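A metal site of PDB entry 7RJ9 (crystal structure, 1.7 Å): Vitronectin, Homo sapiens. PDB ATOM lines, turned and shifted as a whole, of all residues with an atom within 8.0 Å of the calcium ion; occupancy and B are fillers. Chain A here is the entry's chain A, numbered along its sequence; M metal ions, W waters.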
ATOM      1  N   PHE A   9     -19.433  25.574 -21.517  1.00  0.00           N
ATOM      2  CA  PHE A   9     -20.284  26.470 -20.699  1.00  0.00           C
ATOM      3  C   PHE A   9     -21.741  26.095 -20.958  1.00  0.00           C
ATOM      4  O   PHE A   9     -22.073  25.497 -21.984  1.00  0.00           O
ATOM      5  CB  PHE A   9     -20.002  27.942 -20.998  1.00  0.00           C
ATOM      6  CG  PHE A   9     -18.698  28.433 -20.411  1.00  0.00           C
ATOM      7  CD1 PHE A   9     -17.501  28.237 -21.093  1.00  0.00           C
ATOM      8  CD2 PHE A   9     -18.636  28.969 -19.136  1.00  0.00           C
ATOM      9  CE1 PHE A   9     -16.290  28.636 -20.548  1.00  0.00           C
ATOM     10  CE2 PHE A   9     -17.437  29.367 -18.584  1.00  0.00           C
ATOM     11  CZ  PHE A   9     -16.266  29.186 -19.294  1.00  0.00           C
ATOM     12  N   ASP A  10     -22.587  26.482 -20.000  1.00  0.00           N
ATOM     13  CA  ASP A  10     -24.053  26.218 -20.020  1.00  0.00           C
ATOM     14  C   ASP A  10     -24.817  27.426 -20.565  1.00  0.00           C
ATOM     15  O   ASP A  10     -25.849  27.219 -21.232  1.00  0.00           O
ATOM     16  CB  ASP A  10     -24.515  25.902 -18.615  1.00  0.00           C
ATOM     17  CG  ASP A  10     -24.024  24.551 -18.093  1.00  0.00           C
ATOM     18  OD1 ASP A  10     -23.583  23.686 -18.911  1.00  0.00           O
ATOM     19  OD2 ASP A  10     -24.050  24.390 -16.891  1.00  0.00           O
ATOM     20  N   ALA A  11     -24.412  28.642 -20.196  1.00  0.00           N
ATOM     21  CA  ALA A  11     -25.176  29.863 -20.582  1.00  0.00           C
ATOM     22  C   ALA A  11     -24.298  31.084 -20.385  1.00  0.00           C
ATOM     23  O   ALA A  11     -23.370  31.039 -19.571  1.00  0.00           O
ATOM     24  CB  ALA A  11     -26.405  30.000 -19.706  1.00  0.00           C
ATOM     25  N   PHE A  12     -24.643  32.155 -21.096  1.00  0.00           N
ATOM     26  CA  PHE A  12     -24.017  33.483 -20.899  1.00  0.00           C
ATOM     27  C   PHE A  12     -25.123  34.536 -20.902  1.00  0.00           C
ATOM     28  O   PHE A  12     -26.061  34.448 -21.735  1.00  0.00           O
ATOM     29  CB  PHE A  12     -23.040  33.798 -22.035  1.00  0.00           C
ATOM     30  CG  PHE A  12     -21.763  32.990 -22.076  1.00  0.00           C
ATOM     31  CD1 PHE A  12     -21.704  31.804 -22.771  1.00  0.00           C
ATOM     32  CD2 PHE A  12     -20.630  33.413 -21.395  1.00  0.00           C
ATOM     33  CE1 PHE A  12     -20.552  31.045 -22.795  1.00  0.00           C
ATOM     34  CE2 PHE A  12     -19.464  32.665 -21.437  1.00  0.00           C
ATOM     35  CZ  PHE A  12     -19.421  31.476 -22.146  1.00  0.00           C
ATOM     36  N   PHE A  23     -21.993  30.893 -17.078  1.00  0.00           N
ATOM     37  CA  PHE A  23     -22.560  29.847 -16.189  1.00  0.00           C
ATOM     38  C   PHE A  23     -21.970  28.503 -16.574  1.00  0.00           C
ATOM     39  O   PHE A  23     -22.043  28.131 -17.737  1.00  0.00           O
ATOM     40  CB  PHE A  23     -24.098  29.814 -16.268  1.00  0.00           C
ATOM     41  CG  PHE A  23     -24.745  31.068 -15.793  1.00  0.00           C
ATOM     42  CD1 PHE A  23     -25.021  31.269 -14.447  1.00  0.00           C
ATOM     43  CD2 PHE A  23     -25.046  32.096 -16.674  1.00  0.00           C
ATOM     44  CE1 PHE A  23     -25.621  32.428 -14.014  1.00  0.00           C
ATOM     45  CE2 PHE A  23     -25.652  33.261 -16.236  1.00  0.00           C
ATOM     46  CZ  PHE A  23     -25.918  33.436 -14.904  1.00  0.00           C
ATOM     47  N   PRO A  53     -27.729  23.444 -12.765  1.00  0.00           N
ATOM     48  CA  PRO A  53     -27.236  24.268 -13.864  1.00  0.00           C
ATOM     49  C   PRO A  53     -28.359  25.081 -14.535  1.00  0.00           C
ATOM     50  O   PRO A  53     -29.539  24.702 -14.470  1.00  0.00           O
ATOM     51  CB  PRO A  53     -26.652  23.215 -14.796  1.00  0.00           C
ATOM     52  CG  PRO A  53     -27.500  22.014 -14.599  1.00  0.00           C
ATOM     53  CD  PRO A  53     -27.806  22.016 -13.113  1.00  0.00           C
ATOM     54  N   ILE A  54     -28.016  26.173 -15.183  1.00  0.00           N
ATOM     55  CA  ILE A  54     -29.097  26.893 -15.905  1.00  0.00           C
ATOM     56  C   ILE A  54     -28.896  26.639 -17.401  1.00  0.00           C
ATOM     57  O   ILE A  54     -27.703  26.520 -17.855  1.00  0.00           O
ATOM     58  CB  ILE A  54     -29.161  28.372 -15.543  1.00  0.00           C
ATOM     59  CG1 ILE A  54     -28.001  29.113 -16.200  1.00  0.00           C
ATOM     60  CG2 ILE A  54     -29.212  28.575 -14.032  1.00  0.00           C
ATOM     61  CD1 ILE A  54     -28.303  30.542 -16.441  1.00  0.00           C
ATOM     62  N   ASP A  55     -30.001  26.662 -18.128  1.00  0.00           N
ATOM     63  CA  ASP A  55     -30.089  26.289 -19.557  1.00  0.00           C
ATOM     64  C   ASP A  55     -29.595  27.450 -20.418  1.00  0.00           C
ATOM     65  O   ASP A  55     -28.871  27.201 -21.432  1.00  0.00           O
ATOM     66  CB  ASP A  55     -31.525  25.954 -19.962  1.00  0.00           C
ATOM     67  CG  ASP A  55     -32.031  24.661 -19.335  1.00  0.00           C
ATOM     68  OD1 ASP A  55     -31.181  23.840 -18.911  1.00  0.00           O
ATOM     69  OD2 ASP A  55     -33.242  24.499 -19.285  1.00  0.00           O
ATOM     70  N   ALA A  56     -30.064  28.647 -20.124  1.00  0.00           N
ATOM     71  CA  ALA A  56     -29.916  29.812 -21.017  1.00  0.00           C
ATOM     72  C   ALA A  56     -30.097  31.084 -20.214  1.00  0.00           C
ATOM     73  O   ALA A  56     -30.735  31.067 -19.123  1.00  0.00           O
ATOM     74  CB  ALA A  56     -30.917  29.748 -22.141  1.00  0.00           C
ATOM     75  N   ALA A  57     -29.538  32.160 -20.743  1.00  0.00           N
ATOM     76  CA  ALA A  57     -29.682  33.488 -20.125  1.00  0.00           C
ATOM     77  C   ALA A  57     -29.715  34.547 -21.217  1.00  0.00           C
ATOM     78  O   ALA A  57     -29.098  34.364 -22.352  1.00  0.00           O
ATOM     79  CB  ALA A  57     -28.539  33.719 -19.133  1.00  0.00           C
ATOM     80  N   PHE A  70     -32.983  30.855 -17.444  1.00  0.00           N
ATOM     81  CA  PHE A  70     -33.950  29.783 -17.809  1.00  0.00           C
ATOM     82  C   PHE A  70     -33.391  28.444 -17.323  1.00  0.00           C
ATOM     83  O   PHE A  70     -32.179  28.164 -17.476  1.00  0.00           O
ATOM     84  CB  PHE A  70     -34.103  29.693 -19.335  1.00  0.00           C
ATOM     85  CG  PHE A  70     -34.780  30.899 -19.896  1.00  0.00           C
ATOM     86  CD1 PHE A  70     -34.088  32.096 -20.026  1.00  0.00           C
ATOM     87  CD2 PHE A  70     -36.142  30.887 -20.121  1.00  0.00           C
ATOM     88  CE1 PHE A  70     -34.735  33.247 -20.429  1.00  0.00           C
ATOM     89  CE2 PHE A  70     -36.787  32.030 -20.551  1.00  0.00           C
ATOM     90  CZ  PHE A  70     -36.096  33.209 -20.698  1.00  0.00           C
ATOM     91  N   ASN A 101     -36.698  23.696 -21.761  1.00  0.00           N
ATOM     92  CA  ASN A 101     -35.349  23.092 -21.882  1.00  0.00           C
ATOM     93  C   ASN A 101     -34.655  23.669 -23.111  1.00  0.00           C
ATOM     94  O   ASN A 101     -34.104  22.912 -23.927  1.00  0.00           O
ATOM     95  CB  ASN A 101     -35.458  21.579 -21.924  1.00  0.00           C
ATOM     96  CG  ASN A 101     -36.060  21.036 -20.656  1.00  0.00           C
ATOM     97  OD1 ASN A 101     -35.452  21.125 -19.603  1.00  0.00           O
ATOM     98  ND2 ASN A 101     -37.250  20.471 -20.757  1.00  0.00           N
ATOM     99  N   VAL A 102     -34.602  24.982 -23.189  1.00  0.00           N
ATOM    100  CA  VAL A 102     -33.867  25.651 -24.296  1.00  0.00           C
ATOM    101  C   VAL A 102     -32.351  25.396 -24.130  1.00  0.00           C
ATOM    102  O   VAL A 102     -31.879  25.174 -23.049  1.00  0.00           O
ATOM    103  CB  VAL A 102     -34.240  27.121 -24.471  1.00  0.00           C
ATOM    104  CG1 VAL A 102     -35.689  27.281 -24.871  1.00  0.00           C
ATOM    105  CG2 VAL A 102     -33.950  27.948 -23.236  1.00  0.00           C
ATOM    106  N   ASP A 103     -31.642  25.407 -25.253  1.00  0.00           N
ATOM    107  CA  ASP A 103     -30.162  25.270 -25.295  1.00  0.00           C
ATOM    108  C   ASP A 103     -29.462  26.615 -24.982  1.00  0.00           C
ATOM    109  O   ASP A 103     -28.406  26.580 -24.313  1.00  0.00           O
ATOM    110  CB  ASP A 103     -29.754  24.774 -26.671  1.00  0.00           C
ATOM    111  CG  ASP A 103     -30.005  23.295 -26.871  1.00  0.00           C
ATOM    112  OD1 ASP A 103     -30.080  22.577 -25.857  1.00  0.00           O
ATOM    113  OD2 ASP A 103     -30.064  22.898 -28.025  1.00  0.00           O
ATOM    114  N   ALA A 104     -29.995  27.721 -25.476  1.00  0.00           N
ATOM    115  CA  ALA A 104     -29.339  29.049 -25.441  1.00  0.00           C
ATOM    116  C   ALA A 104     -30.336  30.145 -25.747  1.00  0.00           C
ATOM    117  O   ALA A 104     -31.426  29.873 -26.280  1.00  0.00           O
ATOM    118  CB  ALA A 104     -28.206  29.089 -26.448  1.00  0.00           C
ATOM    119  N   ALA A 105     -29.969  31.407 -25.440  1.00  0.00           N
ATOM    120  CA  ALA A 105     -30.765  32.574 -25.773  1.00  0.00           C
ATOM    121  C   ALA A 105     -29.854  33.780 -25.947  1.00  0.00           C
ATOM    122  O   ALA A 105     -28.716  33.779 -25.389  1.00  0.00           O
ATOM    123  CB  ALA A 105     -31.849  32.825 -24.748  1.00  0.00           C
ATOM    124  N   PHE A 122     -32.737  29.230 -28.760  1.00  0.00           N
ATOM    125  CA  PHE A 122     -32.123  28.133 -29.543  1.00  0.00           C
ATOM    126  C   PHE A 122     -32.426  26.823 -28.850  1.00  0.00           C
ATOM    127  O   PHE A 122     -32.182  26.695 -27.631  1.00  0.00           O
ATOM    128  CB  PHE A 122     -30.600  28.347 -29.727  1.00  0.00           C
ATOM    129  CG  PHE A 122     -30.282  29.654 -30.382  1.00  0.00           C
ATOM    130  CD1 PHE A 122     -30.246  30.832 -29.650  1.00  0.00           C
ATOM    131  CD2 PHE A 122     -30.134  29.740 -31.762  1.00  0.00           C
ATOM    132  CE1 PHE A 122     -30.084  32.051 -30.286  1.00  0.00           C
ATOM    133  CE2 PHE A 122     -29.926  30.965 -32.375  1.00  0.00           C
ATOM    134  CZ  PHE A 122     -29.887  32.113 -31.642  1.00  0.00           C
ATOM    135  N   VAL A 156     -26.256  24.454 -30.355  1.00  0.00           N
ATOM    136  CA  VAL A 156     -25.348  25.305 -29.563  1.00  0.00           C
ATOM    137  C   VAL A 156     -25.621  25.028 -28.079  1.00  0.00           C
ATOM    138  O   VAL A 156     -26.698  24.505 -27.721  1.00  0.00           O
ATOM    139  CB  VAL A 156     -25.536  26.787 -29.941  1.00  0.00           C
ATOM    140  CG1 VAL A 156     -25.201  27.054 -31.404  1.00  0.00           C
ATOM    141  CG2 VAL A 156     -26.920  27.327 -29.661  1.00  0.00           C
ATOM    142  N   ASP A 157     -24.674  25.346 -27.235  1.00  0.00           N
ATOM    143  CA  ASP A 157     -24.747  25.145 -25.765  1.00  0.00           C
ATOM    144  C   ASP A 157     -25.108  26.456 -25.070  1.00  0.00           C
ATOM    145  O   ASP A 157     -25.627  26.401 -23.917  1.00  0.00           O
ATOM    146  CB  ASP A 157     -23.393  24.705 -25.233  1.00  0.00           C
ATOM    147  CG  ASP A 157     -22.912  23.354 -25.709  1.00  0.00           C
ATOM    148  OD1 ASP A 157     -23.739  22.536 -26.086  1.00  0.00           O
ATOM    149  OD2 ASP A 157     -21.713  23.120 -25.625  1.00  0.00           O
ATOM    150  N   ALA A 158     -24.764  27.584 -25.684  1.00  0.00           N
ATOM    151  CA  ALA A 158     -24.866  28.925 -25.076  1.00  0.00           C
ATOM    152  C   ALA A 158     -24.701  29.983 -26.165  1.00  0.00           C
ATOM    153  O   ALA A 158     -24.154  29.674 -27.236  1.00  0.00           O
ATOM    154  CB  ALA A 158     -23.837  29.081 -23.978  1.00  0.00           C
ATOM    155  N   ALA A 159     -25.091  31.214 -25.885  1.00  0.00           N
ATOM    156  CA  ALA A 159     -24.967  32.316 -26.842  1.00  0.00           C
ATOM    157  C   ALA A 159     -24.903  33.629 -26.076  1.00  0.00           C
ATOM    158  O   ALA A 159     -25.396  33.696 -24.951  1.00  0.00           O
ATOM    159  CB  ALA A 159     -26.114  32.292 -27.844  1.00  0.00           C
ATOM    160  N   PHE A 169     -21.563  29.223 -28.660  1.00  0.00           N
ATOM    161  CA  PHE A 169     -20.670  28.325 -27.901  1.00  0.00           C
ATOM    162  C   PHE A 169     -21.165  26.885 -28.124  1.00  0.00           C
ATOM    163  O   PHE A 169     -22.359  26.610 -27.973  1.00  0.00           O
ATOM    164  CB  PHE A 169     -20.587  28.727 -26.436  1.00  0.00           C
ATOM    165  CG  PHE A 169     -20.157  30.157 -26.213  1.00  0.00           C
ATOM    166  CD1 PHE A 169     -21.083  31.194 -26.232  1.00  0.00           C
ATOM    167  CD2 PHE A 169     -18.813  30.490 -26.042  1.00  0.00           C
ATOM    168  CE1 PHE A 169     -20.696  32.504 -26.041  1.00  0.00           C
ATOM    169  CE2 PHE A 169     -18.440  31.803 -25.830  1.00  0.00           C
ATOM    170  CZ  PHE A 169     -19.373  32.823 -25.837  1.00  0.00           C
HETATM  171 CA    CA M   1     -27.290  25.777 -22.403  1.00  0.00          CA
HETATM  172  O   HOH W   1     -26.287  23.597 -22.958  1.00  0.00           O
HETATM  173  O   HOH W   2     -27.082  24.677 -20.158  1.00  0.00           O
HETATM  174  O   HOH W   3     -29.315  24.331 -22.247  1.00  0.00           O
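N of Asp 157 is in hydrogen-bond range of O of Phe 169 (2.7 Å). N of Asp 55 lies within hydrogen-bond range of O of Phe 70 (2.7 Å). N of Asp 10 sits at hydrogen-bond distance from O of Phe 23. O of Phe 122 sits at hydrogen-bond distance from N of Asp 103 (2.8 Å).
Four residues have an atom within 4 Å of the calcium ion: Asp 10, Asp 55, Asp 103 and Asp 157.
The calcium ion is bound by the backbone carbonyl oxygen (O) of Asp 157, the backbone carbonyl oxygen (O) of Asp 55, the backbone carbonyl oxygen (O) of Asp 10, the backbone carbonyl oxygen (O) of Asp 103, water W1, water W3 and water W2. The calcium ion has seven donor atoms within binding distance.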
